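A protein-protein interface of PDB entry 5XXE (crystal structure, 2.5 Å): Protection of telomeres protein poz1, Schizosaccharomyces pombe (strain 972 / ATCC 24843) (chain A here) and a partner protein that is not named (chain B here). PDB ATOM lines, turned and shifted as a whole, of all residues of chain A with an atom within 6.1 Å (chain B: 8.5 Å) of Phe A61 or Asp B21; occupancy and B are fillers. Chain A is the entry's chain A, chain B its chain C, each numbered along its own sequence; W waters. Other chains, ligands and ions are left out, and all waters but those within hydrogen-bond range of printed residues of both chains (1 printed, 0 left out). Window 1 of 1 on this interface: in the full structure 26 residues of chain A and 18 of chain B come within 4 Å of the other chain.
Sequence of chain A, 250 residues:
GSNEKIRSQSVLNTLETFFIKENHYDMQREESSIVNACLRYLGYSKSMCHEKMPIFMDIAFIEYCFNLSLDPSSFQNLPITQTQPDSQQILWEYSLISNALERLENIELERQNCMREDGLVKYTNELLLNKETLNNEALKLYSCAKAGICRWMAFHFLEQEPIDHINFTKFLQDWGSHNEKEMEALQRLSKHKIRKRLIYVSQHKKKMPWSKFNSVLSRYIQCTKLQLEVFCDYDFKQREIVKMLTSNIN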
ATOM      1  N   PHE A  19     -28.700   1.163  27.506  1.00  0.00           N
ATOM      2  CA  PHE A  19     -29.809   0.805  26.598  1.00  0.00           C
ATOM      3  C   PHE A  19     -31.205   0.896  27.211  1.00  0.00           C
ATOM      4  O   PHE A  19     -32.128   1.383  26.563  1.00  0.00           O
ATOM      5  CB  PHE A  19     -29.634  -0.618  26.053  1.00  0.00           C
ATOM      6  CG  PHE A  19     -28.663  -0.748  24.911  1.00  0.00           C
ATOM      7  CD1 PHE A  19     -28.040   0.348  24.318  1.00  0.00           C
ATOM      8  CD2 PHE A  19     -28.410  -2.006  24.390  1.00  0.00           C
ATOM      9  CE1 PHE A  19     -27.170   0.179  23.257  1.00  0.00           C
ATOM     10  CE2 PHE A  19     -27.543  -2.180  23.325  1.00  0.00           C
ATOM     11  CZ  PHE A  19     -26.921  -1.083  22.756  1.00  0.00           C
ATOM     12  N   PHE A  56     -33.500  -7.011  26.637  1.00  0.00           N
ATOM     13  CA  PHE A  56     -33.198  -5.574  26.496  1.00  0.00           C
ATOM     14  C   PHE A  56     -32.341  -5.258  25.265  1.00  0.00           C
ATOM     15  O   PHE A  56     -32.361  -4.130  24.787  1.00  0.00           O
ATOM     16  CB  PHE A  56     -32.547  -4.989  27.769  1.00  0.00           C
ATOM     17  CG  PHE A  56     -31.048  -5.177  27.854  1.00  0.00           C
ATOM     18  CD1 PHE A  56     -30.178  -4.279  27.231  1.00  0.00           C
ATOM     19  CD2 PHE A  56     -30.502  -6.232  28.581  1.00  0.00           C
ATOM     20  CE1 PHE A  56     -28.801  -4.455  27.301  1.00  0.00           C
ATOM     21  CE2 PHE A  56     -29.125  -6.403  28.663  1.00  0.00           C
ATOM     22  CZ  PHE A  56     -28.275  -5.514  28.025  1.00  0.00           C
ATOM     23  N   MET A  57     -31.576  -6.236  24.774  1.00  0.00           N
ATOM     24  CA  MET A  57     -30.758  -6.058  23.570  1.00  0.00           C
ATOM     25  C   MET A  57     -31.644  -5.996  22.359  1.00  0.00           C
ATOM     26  O   MET A  57     -31.501  -5.095  21.528  1.00  0.00           O
ATOM     27  CB  MET A  57     -29.746  -7.188  23.371  1.00  0.00           C
ATOM     28  CG  MET A  57     -28.733  -7.319  24.512  1.00  0.00           C
ATOM     29  SD  MET A  57     -27.379  -5.895  24.429  1.00  0.00           S
ATOM     30  CE  MET A  57     -26.223  -6.707  23.059  1.00  0.00           C
ATOM     31  N   ASP A  58     -32.578  -6.942  22.256  1.00  0.00           N
ATOM     32  CA  ASP A  58     -33.538  -6.956  21.147  1.00  0.00           C
ATOM     33  C   ASP A  58     -34.399  -5.681  21.138  1.00  0.00           C
ATOM     34  O   ASP A  58     -34.583  -5.070  20.086  1.00  0.00           O
ATOM     35  CB  ASP A  58     -34.431  -8.200  21.197  1.00  0.00           C
ATOM     36  CG  ASP A  58     -33.638  -9.496  21.143  1.00  0.00           C
ATOM     37  OD1 ASP A  58     -33.214  -9.965  22.221  1.00  0.00           O
ATOM     38  OD2 ASP A  58     -33.443 -10.043  20.033  1.00  0.00           O
ATOM     39  N   ILE A  59     -34.884  -5.265  22.310  1.00  0.00           N
ATOM     40  CA  ILE A  59     -35.675  -4.033  22.428  1.00  0.00           C
ATOM     41  C   ILE A  59     -34.880  -2.796  21.983  1.00  0.00           C
ATOM     42  O   ILE A  59     -35.385  -1.965  21.219  1.00  0.00           O
ATOM     43  CB  ILE A  59     -36.210  -3.824  23.866  1.00  0.00           C
ATOM     44  CG1 ILE A  59     -37.259  -4.892  24.209  1.00  0.00           C
ATOM     45  CG2 ILE A  59     -36.821  -2.431  24.030  1.00  0.00           C
ATOM     46  CD1 ILE A  59     -37.482  -5.079  25.695  1.00  0.00           C
ATOM     47  N   ALA A  60     -33.644  -2.674  22.457  1.00  0.00           N
ATOM     48  CA  ALA A  60     -32.803  -1.548  22.060  1.00  0.00           C
ATOM     49  C   ALA A  60     -32.552  -1.564  20.555  1.00  0.00           C
ATOM     50  O   ALA A  60     -32.536  -0.505  19.915  1.00  0.00           O
ATOM     51  CB  ALA A  60     -31.489  -1.560  22.823  1.00  0.00           C
ATOM     52  N   PHE A  61     -32.372  -2.757  19.992  1.00  0.00           N
ATOM     53  CA  PHE A  61     -32.231  -2.883  18.549  1.00  0.00           C
ATOM     54  C   PHE A  61     -33.487  -2.400  17.807  1.00  0.00           C
ATOM     55  O   PHE A  61     -33.380  -1.634  16.849  1.00  0.00           O
ATOM     56  CB  PHE A  61     -31.892  -4.313  18.118  1.00  0.00           C
ATOM     57  CG  PHE A  61     -31.713  -4.445  16.635  1.00  0.00           C
ATOM     58  CD1 PHE A  61     -30.524  -4.079  16.039  1.00  0.00           C
ATOM     59  CD2 PHE A  61     -32.765  -4.870  15.824  1.00  0.00           C
ATOM     60  CE1 PHE A  61     -30.364  -4.164  14.669  1.00  0.00           C
ATOM     61  CE2 PHE A  61     -32.615  -4.953  14.447  1.00  0.00           C
ATOM     62  CZ  PHE A  61     -31.412  -4.600  13.870  1.00  0.00           C
ATOM     63  N   ILE A  62     -34.665  -2.844  18.243  1.00  0.00           N
ATOM     64  CA  ILE A  62     -35.921  -2.439  17.599  1.00  0.00           C
ATOM     65  C   ILE A  62     -36.093  -0.920  17.713  1.00  0.00           C
ATOM     66  O   ILE A  62     -36.411  -0.251  16.723  1.00  0.00           O
ATOM     67  CB  ILE A  62     -37.152  -3.190  18.181  1.00  0.00           C
ATOM     68  CG1 ILE A  62     -37.087  -4.694  17.873  1.00  0.00           C
ATOM     69  CG2 ILE A  62     -38.458  -2.613  17.652  1.00  0.00           C
ATOM     70  CD1 ILE A  62     -36.904  -5.045  16.417  1.00  0.00           C
ATOM     71  N   GLU A  63     -35.852  -0.382  18.904  1.00  0.00           N
ATOM     72  CA  GLU A  63     -35.900   1.071  19.113  1.00  0.00           C
ATOM     73  C   GLU A  63     -34.930   1.804  18.186  1.00  0.00           C
ATOM     74  O   GLU A  63     -35.296   2.807  17.565  1.00  0.00           O
ATOM     75  CB  GLU A  63     -35.637   1.416  20.582  1.00  0.00           C
ATOM     76  CG  GLU A  63     -36.781   1.011  21.515  1.00  0.00           C
ATOM     77  CD  GLU A  63     -36.491   1.234  22.996  1.00  0.00           C
ATOM     78  OE1 GLU A  63     -35.313   1.164  23.426  1.00  0.00           O
ATOM     79  OE2 GLU A  63     -37.457   1.492  23.754  1.00  0.00           O
ATOM     80  N   TYR A  64     -33.713   1.275  18.061  1.00  0.00           N
ATOM     81  CA  TYR A  64     -32.695   1.845  17.168  1.00  0.00           C
ATOM     82  C   TYR A  64     -33.006   1.650  15.677  1.00  0.00           C
ATOM     83  O   TYR A  64     -32.886   2.599  14.891  1.00  0.00           O
ATOM     84  CB  TYR A  64     -31.314   1.256  17.492  1.00  0.00           C
ATOM     85  CG  TYR A  64     -30.202   1.821  16.646  1.00  0.00           C
ATOM     86  CD1 TYR A  64     -29.962   3.185  16.621  1.00  0.00           C
ATOM     87  CD2 TYR A  64     -29.397   0.999  15.864  1.00  0.00           C
ATOM     88  CE1 TYR A  64     -28.964   3.721  15.834  1.00  0.00           C
ATOM     89  CE2 TYR A  64     -28.379   1.529  15.087  1.00  0.00           C
ATOM     90  CZ  TYR A  64     -28.167   2.893  15.086  1.00  0.00           C
ATOM     91  OH  TYR A  64     -27.175   3.451  14.320  1.00  0.00           O
ATOM     92  N   CYS A  65     -33.395   0.427  15.301  1.00  0.00           N
ATOM     93  CA  CYS A  65     -33.663   0.054  13.899  1.00  0.00           C
ATOM     94  C   CYS A  65     -34.776   0.867  13.254  1.00  0.00           C
ATOM     95  O   CYS A  65     -34.665   1.247  12.084  1.00  0.00           O
ATOM     96  CB  CYS A  65     -34.030  -1.425  13.789  1.00  0.00           C
ATOM     97  SG  CYS A  65     -34.263  -1.999  12.090  1.00  0.00           S
ATOM     98  N   PHE A  66     -35.834   1.132  14.023  1.00  0.00           N
ATOM     99  CA  PHE A  66     -36.999   1.881  13.536  1.00  0.00           C
ATOM    100  C   PHE A  66     -37.097   3.311  14.080  1.00  0.00           C
ATOM    101  O   PHE A  66     -38.168   3.910  14.040  1.00  0.00           O
ATOM    102  CB  PHE A  66     -38.266   1.073  13.813  1.00  0.00           C
ATOM    103  CG  PHE A  66     -38.268  -0.258  13.124  1.00  0.00           C
ATOM    104  CD1 PHE A  66     -38.475  -0.336  11.753  1.00  0.00           C
ATOM    105  CD2 PHE A  66     -38.012  -1.425  13.824  1.00  0.00           C
ATOM    106  CE1 PHE A  66     -38.454  -1.558  11.096  1.00  0.00           C
ATOM    107  CE2 PHE A  66     -37.986  -2.648  13.179  1.00  0.00           C
ATOM    108  CZ  PHE A  66     -38.209  -2.717  11.808  1.00  0.00           C
ATOM    109  N   SER A  95     -32.347  -8.702   4.371  1.00  0.00           N
ATOM    110  CA  SER A  95     -31.670  -9.394   5.478  1.00  0.00           C
ATOM    111  C   SER A  95     -31.823  -8.672   6.829  1.00  0.00           C
ATOM    112  O   SER A  95     -32.050  -9.311   7.856  1.00  0.00           O
ATOM    113  CB  SER A  95     -30.187  -9.581   5.154  1.00  0.00           C
ATOM    114  OG  SER A  95     -29.588 -10.498   6.048  1.00  0.00           O
ATOM    115  N   LEU A  96     -31.727  -7.343   6.812  1.00  0.00           N
ATOM    116  CA  LEU A  96     -31.803  -6.545   8.033  1.00  0.00           C
ATOM    117  C   LEU A  96     -33.186  -6.565   8.668  1.00  0.00           C
ATOM    118  O   LEU A  96     -33.306  -6.774   9.879  1.00  0.00           O
ATOM    119  CB  LEU A  96     -31.400  -5.090   7.752  1.00  0.00           C
ATOM    120  CG  LEU A  96     -31.462  -4.143   8.954  1.00  0.00           C
ATOM    121  CD1 LEU A  96     -30.386  -4.516   9.968  1.00  0.00           C
ATOM    122  CD2 LEU A  96     -31.331  -2.692   8.525  1.00  0.00           C
ATOM    123  N   ASN A  99     -34.128 -10.016  10.041  1.00  0.00           N
ATOM    124  CA  ASN A  99     -33.521 -10.113  11.380  1.00  0.00           C
ATOM    125  C   ASN A  99     -34.230  -9.233  12.410  1.00  0.00           C
ATOM    126  O   ASN A  99     -34.397  -9.641  13.554  1.00  0.00           O
ATOM    127  CB  ASN A  99     -32.045  -9.714  11.337  1.00  0.00           C
ATOM    128  CG  ASN A  99     -31.172 -10.728  10.628  1.00  0.00           C
ATOM    129  OD1 ASN A  99     -31.638 -11.759  10.149  1.00  0.00           O
ATOM    130  ND2 ASN A  99     -29.880 -10.434  10.565  1.00  0.00           N
ATOM    131  N   ALA A 100     -34.636  -8.031  12.004  1.00  0.00           N
ATOM    132  CA  ALA A 100     -35.398  -7.140  12.878  1.00  0.00           C
ATOM    133  C   ALA A 100     -36.720  -7.771  13.308  1.00  0.00           C
ATOM    134  O   ALA A 100     -37.049  -7.758  14.493  1.00  0.00           O
ATOM    135  CB  ALA A 100     -35.643  -5.795  12.201  1.00  0.00           C
ATOM    136  N   ARG A 103     -36.159 -10.500  15.834  1.00  0.00           N
ATOM    137  CA  ARG A 103     -35.919  -9.967  17.188  1.00  0.00           C
ATOM    138  C   ARG A 103     -37.203  -9.433  17.824  1.00  0.00           C
ATOM    139  O   ARG A 103     -37.406  -9.580  19.038  1.00  0.00           O
ATOM    140  CB  ARG A 103     -34.815  -8.902  17.182  1.00  0.00           C
ATOM    141  CG  ARG A 103     -33.456  -9.486  16.837  1.00  0.00           C
ATOM    142  CD  ARG A 103     -32.287  -8.545  17.095  1.00  0.00           C
ATOM    143  NE  ARG A 103     -31.066  -9.090  16.485  1.00  0.00           N
ATOM    144  CZ  ARG A 103     -30.612  -8.815  15.258  1.00  0.00           C
ATOM    145  NH1 ARG A 103     -31.234  -7.949  14.457  1.00  0.00           N
ATOM    146  NH2 ARG A 103     -29.503  -9.405  14.826  1.00  0.00           N
ATOM    147  N   SER B  14     -25.746 -14.822  18.320  1.00  0.00           N
ATOM    148  CA  SER B  14     -26.658 -13.676  18.401  1.00  0.00           C
ATOM    149  C   SER B  14     -25.953 -12.326  18.489  1.00  0.00           C
ATOM    150  O   SER B  14     -26.364 -11.369  17.826  1.00  0.00           O
ATOM    151  CB  SER B  14     -27.585 -13.803  19.609  1.00  0.00           C
ATOM    152  OG  SER B  14     -28.392 -14.951  19.501  1.00  0.00           O
ATOM    153  N   PHE B  15     -24.915 -12.252  19.323  1.00  0.00           N
ATOM    154  CA  PHE B  15     -24.211 -10.994  19.571  1.00  0.00           C
ATOM    155  C   PHE B  15     -23.453 -10.515  18.348  1.00  0.00           C
ATOM    156  O   PHE B  15     -23.408  -9.308  18.087  1.00  0.00           O
ATOM    157  CB  PHE B  15     -23.275 -11.106  20.779  1.00  0.00           C
ATOM    158  CG  PHE B  15     -24.000 -11.188  22.085  1.00  0.00           C
ATOM    159  CD1 PHE B  15     -24.459 -10.030  22.712  1.00  0.00           C
ATOM    160  CD2 PHE B  15     -24.257 -12.418  22.678  1.00  0.00           C
ATOM    161  CE1 PHE B  15     -25.143 -10.099  23.915  1.00  0.00           C
ATOM    162  CE2 PHE B  15     -24.946 -12.492  23.879  1.00  0.00           C
ATOM    163  CZ  PHE B  15     -25.389 -11.330  24.501  1.00  0.00           C
ATOM    164  N   PHE B  16     -22.866 -11.451  17.603  1.00  0.00           N
ATOM    165  CA  PHE B  16     -22.194 -11.107  16.357  1.00  0.00           C
ATOM    166  C   PHE B  16     -23.168 -10.595  15.298  1.00  0.00           C
ATOM    167  O   PHE B  16     -22.876  -9.614  14.605  1.00  0.00           O
ATOM    168  CB  PHE B  16     -21.423 -12.297  15.783  1.00  0.00           C
ATOM    169  CG  PHE B  16     -20.701 -11.973  14.505  1.00  0.00           C
ATOM    170  CD1 PHE B  16     -19.730 -10.983  14.483  1.00  0.00           C
ATOM    171  CD2 PHE B  16     -21.019 -12.618  13.321  1.00  0.00           C
ATOM    172  CE1 PHE B  16     -19.064 -10.663  13.308  1.00  0.00           C
ATOM    173  CE2 PHE B  16     -20.361 -12.304  12.141  1.00  0.00           C
ATOM    174  CZ  PHE B  16     -19.381 -11.326  12.133  1.00  0.00           C
ATOM    175  N   GLU B  17     -24.305 -11.276  15.160  1.00  0.00           N
ATOM    176  CA  GLU B  17     -25.300 -10.917  14.155  1.00  0.00           C
ATOM    177  C   GLU B  17     -25.937  -9.579  14.507  1.00  0.00           C
ATOM    178  O   GLU B  17     -26.135  -8.742  13.628  1.00  0.00           O
ATOM    179  CB  GLU B  17     -26.361 -12.019  13.993  1.00  0.00           C
ATOM    180  CG  GLU B  17     -25.827 -13.349  13.443  1.00  0.00           C
ATOM    181  CD  GLU B  17     -25.252 -13.247  12.033  1.00  0.00           C
ATOM    182  OE1 GLU B  17     -25.951 -12.738  11.123  1.00  0.00           O
ATOM    183  OE2 GLU B  17     -24.095 -13.684  11.828  1.00  0.00           O
ATOM    184  N   LEU B  18     -26.223  -9.369  15.789  1.00  0.00           N
ATOM    185  CA  LEU B  18     -26.650  -8.060  16.284  1.00  0.00           C
ATOM    186  C   LEU B  18     -25.637  -6.972  15.921  1.00  0.00           C
ATOM    187  O   LEU B  18     -26.027  -5.908  15.424  1.00  0.00           O
ATOM    188  CB  LEU B  18     -26.829  -8.078  17.795  1.00  0.00           C
ATOM    189  CG  LEU B  18     -27.401  -6.772  18.358  1.00  0.00           C
ATOM    190  CD1 LEU B  18     -28.904  -6.880  18.459  1.00  0.00           C
ATOM    191  CD2 LEU B  18     -26.815  -6.446  19.717  1.00  0.00           C
ATOM    192  N   LEU B  19     -24.353  -7.248  16.161  1.00  0.00           N
ATOM    193  CA  LEU B  19     -23.281  -6.330  15.787  1.00  0.00           C
ATOM    194  C   LEU B  19     -23.335  -5.957  14.311  1.00  0.00           C
ATOM    195  O   LEU B  19     -23.302  -4.774  13.975  1.00  0.00           O
ATOM    196  CB  LEU B  19     -21.895  -6.897  16.138  1.00  0.00           C
ATOM    197  CG  LEU B  19     -20.664  -6.160  15.583  1.00  0.00           C
ATOM    198  CD1 LEU B  19     -20.548  -4.782  16.209  1.00  0.00           C
ATOM    199  CD2 LEU B  19     -19.407  -6.980  15.808  1.00  0.00           C
ATOM    200  N   ARG B  20     -23.403  -6.954  13.436  1.00  0.00           N
ATOM    201  CA  ARG B  20     -23.445  -6.684  11.995  1.00  0.00           C
ATOM    202  C   ARG B  20     -24.639  -5.828  11.596  1.00  0.00           C
ATOM    203  O   ARG B  20     -24.490  -4.897  10.805  1.00  0.00           O
ATOM    204  CB  ARG B  20     -23.447  -7.970  11.184  1.00  0.00           C
ATOM    205  CG  ARG B  20     -22.071  -8.581  11.020  1.00  0.00           C
ATOM    206  CD  ARG B  20     -22.154  -9.918  10.303  1.00  0.00           C
ATOM    207  NE  ARG B  20     -22.725  -9.765   8.966  1.00  0.00           N
ATOM    208  CZ  ARG B  20     -23.228 -10.754   8.226  1.00  0.00           C
ATOM    209  NH1 ARG B  20     -23.245 -12.019   8.673  1.00  0.00           N
ATOM    210  NH2 ARG B  20     -23.729 -10.470   7.021  1.00  0.00           N
ATOM    211  N   ASP B  21     -25.805  -6.130  12.163  1.00  0.00           N
ATOM    212  CA  ASP B  21     -27.036  -5.395  11.843  1.00  0.00           C
ATOM    213  C   ASP B  21     -26.976  -3.961  12.348  1.00  0.00           C
ATOM    214  O   ASP B  21     -27.378  -3.032  11.654  1.00  0.00           O
ATOM    215  CB  ASP B  21     -28.272  -6.101  12.427  1.00  0.00           C
ATOM    216  CG  ASP B  21     -28.541  -7.454  11.782  1.00  0.00           C
ATOM    217  OD1 ASP B  21     -27.920  -7.774  10.741  1.00  0.00           O
ATOM    218  OD2 ASP B  21     -29.373  -8.213  12.334  1.00  0.00           O
ATOM    219  N   TRP B  22     -26.466  -3.799  13.561  1.00  0.00           N
ATOM    220  CA  TRP B  22     -26.280  -2.481  14.158  1.00  0.00           C
ATOM    221  C   TRP B  22     -25.337  -1.619  13.318  1.00  0.00           C
ATOM    222  O   TRP B  22     -25.616  -0.445  13.095  1.00  0.00           O
ATOM    223  CB  TRP B  22     -25.765  -2.613  15.587  1.00  0.00           C
ATOM    224  CG  TRP B  22     -25.979  -1.404  16.402  1.00  0.00           C
ATOM    225  CD1 TRP B  22     -25.302  -0.230  16.317  1.00  0.00           C
ATOM    226  CD2 TRP B  22     -26.923  -1.252  17.459  1.00  0.00           C
ATOM    227  NE1 TRP B  22     -25.777   0.655  17.249  1.00  0.00           N
ATOM    228  CE2 TRP B  22     -26.774   0.053  17.963  1.00  0.00           C
ATOM    229  CE3 TRP B  22     -27.884  -2.093  18.029  1.00  0.00           C
ATOM    230  CZ2 TRP B  22     -27.547   0.541  19.005  1.00  0.00           C
ATOM    231  CZ3 TRP B  22     -28.660  -1.607  19.071  1.00  0.00           C
ATOM    232  CH2 TRP B  22     -28.485  -0.302  19.548  1.00  0.00           C
ATOM    233  N   LYS B  23     -24.251  -2.213  12.829  1.00  0.00           N
ATOM    234  CA  LYS B  23     -23.310  -1.501  11.950  1.00  0.00           C
ATOM    235  C   LYS B  23     -23.937  -1.071  10.625  1.00  0.00           C
ATOM    236  O   LYS B  23     -23.675   0.031  10.157  1.00  0.00           O
ATOM    237  CB  LYS B  23     -22.052  -2.340  11.681  1.00  0.00           C
ATOM    238  CG  LYS B  23     -21.071  -2.372  12.845  1.00  0.00           C
ATOM    239  CD  LYS B  23     -20.204  -1.121  12.865  1.00  0.00           C
ATOM    240  CE  LYS B  23     -19.766  -0.748  14.273  1.00  0.00           C
ATOM    241  NZ  LYS B  23     -19.026   0.545  14.272  1.00  0.00           N
ATOM    242  N   LYS B  24     -24.753  -1.936  10.021  1.00  0.00           N
ATOM    243  CA  LYS B  24     -25.462  -1.595   8.770  1.00  0.00           C
ATOM    244  C   LYS B  24     -26.310  -0.333   8.924  1.00  0.00           C
ATOM    245  O   LYS B  24     -26.277   0.547   8.074  1.00  0.00           O
ATOM    246  CB  LYS B  24     -26.365  -2.743   8.308  1.00  0.00           C
ATOM    247  CG  LYS B  24     -25.638  -3.940   7.711  1.00  0.00           C
ATOM    248  CD  LYS B  24     -26.640  -4.916   7.111  1.00  0.00           C
ATOM    249  CE  LYS B  24     -26.082  -6.318   6.993  1.00  0.00           C
ATOM    250  NZ  LYS B  24     -27.140  -7.248   6.508  1.00  0.00           N
ATOM    251  N   ILE B  25     -27.050  -0.257  10.024  1.00  0.00           N
ATOM    252  CA  ILE B  25     -27.907   0.878  10.302  1.00  0.00           C
ATOM    253  C   ILE B  25     -27.064   2.147  10.451  1.00  0.00           C
ATOM    254  O   ILE B  25     -27.458   3.206   9.951  1.00  0.00           O
ATOM    255  CB  ILE B  25     -28.777   0.641  11.562  1.00  0.00           C
ATOM    256  CG1 ILE B  25     -29.738  -0.531  11.341  1.00  0.00           C
ATOM    257  CG2 ILE B  25     -29.571   1.894  11.921  1.00  0.00           C
ATOM    258  CD1 ILE B  25     -30.282  -1.136  12.616  1.00  0.00           C
ATOM    259  N   GLU B  26     -25.914   2.034  11.129  1.00  0.00           N
ATOM    260  CA  GLU B  26     -24.988   3.161  11.318  1.00  0.00           C
ATOM    261  C   GLU B  26     -24.415   3.666  10.013  1.00  0.00           C
ATOM    262  O   GLU B  26     -24.470   4.862   9.737  1.00  0.00           O
ATOM    263  CB  GLU B  26     -23.824   2.777  12.230  1.00  0.00           C
ATOM    264  CG  GLU B  26     -24.216   2.664  13.685  1.00  0.00           C
ATOM    265  CD  GLU B  26     -23.062   2.323  14.600  1.00  0.00           C
ATOM    266  OE1 GLU B  26     -23.218   2.582  15.801  1.00  0.00           O
ATOM    267  OE2 GLU B  26     -22.020   1.807  14.138  1.00  0.00           O
ATOM    268  N   GLU B  27     -23.842   2.754   9.234  1.00  0.00           N
ATOM    269  CA  GLU B  27     -23.305   3.076   7.909  1.00  0.00           C
ATOM    270  C   GLU B  27     -24.357   3.809   7.066  1.00  0.00           C
ATOM    271  O   GLU B  27     -24.038   4.798   6.410  1.00  0.00           O
ATOM    272  CB  GLU B  27     -22.801   1.796   7.208  1.00  0.00           C
ATOM    273  CG  GLU B  27     -22.380   1.922   5.736  1.00  0.00           C
ATOM    274  CD  GLU B  27     -21.001   2.554   5.514  1.00  0.00           C
ATOM    275  OE1 GLU B  27     -20.478   3.261   6.409  1.00  0.00           O
ATOM    276  OE2 GLU B  27     -20.435   2.345   4.415  1.00  0.00           O
ATOM    277  N   PHE B  28     -25.605   3.339   7.118  1.00  0.00           N
ATOM    278  CA  PHE B  28     -26.708   3.959   6.381  1.00  0.00           C
ATOM    279  C   PHE B  28     -27.029   5.374   6.872  1.00  0.00           C
ATOM    280  O   PHE B  28     -27.209   6.277   6.057  1.00  0.00           O
ATOM    281  CB  PHE B  28     -27.968   3.076   6.437  1.00  0.00           C
ATOM    282  CG  PHE B  28     -29.174   3.692   5.771  1.00  0.00           C
ATOM    283  CD1 PHE B  28     -29.262   3.754   4.384  1.00  0.00           C
ATOM    284  CD2 PHE B  28     -30.217   4.225   6.532  1.00  0.00           C
ATOM    285  CE1 PHE B  28     -30.367   4.329   3.769  1.00  0.00           C
ATOM    286  CE2 PHE B  28     -31.325   4.800   5.918  1.00  0.00           C
ATOM    287  CZ  PHE B  28     -31.397   4.852   4.535  1.00  0.00           C
ATOM    288  N   ARG B  29     -27.106   5.561   8.187  1.00  0.00           N
ATOM    289  CA  ARG B  29     -27.406   6.878   8.777  1.00  0.00           C
ATOM    290  C   ARG B  29     -26.242   7.900   8.800  1.00  0.00           C
ATOM    291  O   ARG B  29     -26.483   9.074   9.071  1.00  0.00           O
ATOM    292  CB  ARG B  29     -27.967   6.706  10.194  1.00  0.00           C
ATOM    293  CG  ARG B  29     -29.322   6.029  10.208  1.00  0.00           C
ATOM    294  CD  ARG B  29     -29.889   5.819  11.604  1.00  0.00           C
ATOM    295  NE  ARG B  29     -31.094   4.989  11.547  1.00  0.00           N
ATOM    296  CZ  ARG B  29     -31.743   4.491  12.599  1.00  0.00           C
ATOM    297  NH1 ARG B  29     -31.323   4.717  13.843  1.00  0.00           N
ATOM    298  NH2 ARG B  29     -32.831   3.748  12.404  1.00  0.00           N
HETATM  299  O   HOH W   1     -29.047 -11.251  17.037  1.00  0.00           O
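The backbone carbonyl oxygen of Ser A95 sits close to the side-chain amide oxygen of Asn A99.
The side-chain carboxylate (OE2) of Glu B17 is in salt-bridge range of the guanidinium group (NH1) of Arg B20 (3.7 Å).
The side-chain carboxylate (OE2) of Glu B26 is in salt-bridge range of the side-chain amino group (NZ) of Lys B23 (3.3 Å).
Among the printed residues, merely in contact across the chains: Phe A19 with Trp B22 (3.7 Å), Met A57 with Phe B15 (3.7 Å), Met A57 with Leu B18 (3.4 Å), Phe A61 with Leu B18 (3.95 Å), Phe A61 with Asp B21 (3.6 Å), Phe A61 with Trp B22 (3.8 Å), Phe A61 with Ile B25 (3.7 Å), Tyr A64 with Trp B22 (3.5 Å), Tyr A64 with Ile B25 (3.4 Å), Tyr A64 with Glu B26 (3.1 Å), Cys A65 with Ile B25 (3.8 Å), Leu A96 with Asp B21 (3.6 Å), Leu A96 with Ile B25 (3.9 Å) and Arg A103 with Glu B17 (3.6 Å).
Hydrophobic or aromatic side chains of chain A within 4 Å of the printed part of chain B: Phe A19, Met A57, Phe A61, Tyr A64 and Leu A96.
Among the printed residues, 19 pairs touch across the chains.
O of Tyr A64 lies within hydrogen-bond range of NH2 of Arg B29.
O of Cys A65 is in hydrogen-bond range of NH2 of Arg B29.
OD2 of Asp B21 lies within hydrogen-bond range of ND2 of Asn A99 (2.9 Å).
OD2 of Asp B21 lies within salt-bridge range of NH2 of Arg A103, at 2.8 Å.
N of Leu B18 sits close to NH2 of Arg A103 (3.4 Å).
Of the printed residues of chain B, Met A57 touches Phe B15 (3.7 Å) and Leu B18 (3.4 Å).
No residue of chain B comes within 4 Å of Ala A60.
Printed residues of chain B within 4 Å of Phe A61: Leu B18, Asp B21, Trp B22 and Ile B25.
Of the printed residues of chain B, Asn A99 touches Asp B21.
Ala A100 touches none of the printed residues of chain B.
Printed residues of chain A within 4 Å of Asp B21: Phe A61, Leu A96, Asn A99 and Arg A103.
The nearest residue of chain B that does not touch Phe A61 is Glu B17 (6.3 Å).
The nearest printed residue of chain A that does not touch Asp B21 is Ser A95 (5.3 Å).
The nearest printed residue of chain B that does not touch Asn A99 is Glu B17 (4.6 Å).
Water W1 lies within hydrogen-bond range of the backbone carbonyl oxygen (O) of Ser B14 (2.8 Å) and the guanidinium group (NH2) of Arg A103 (2.9 Å).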
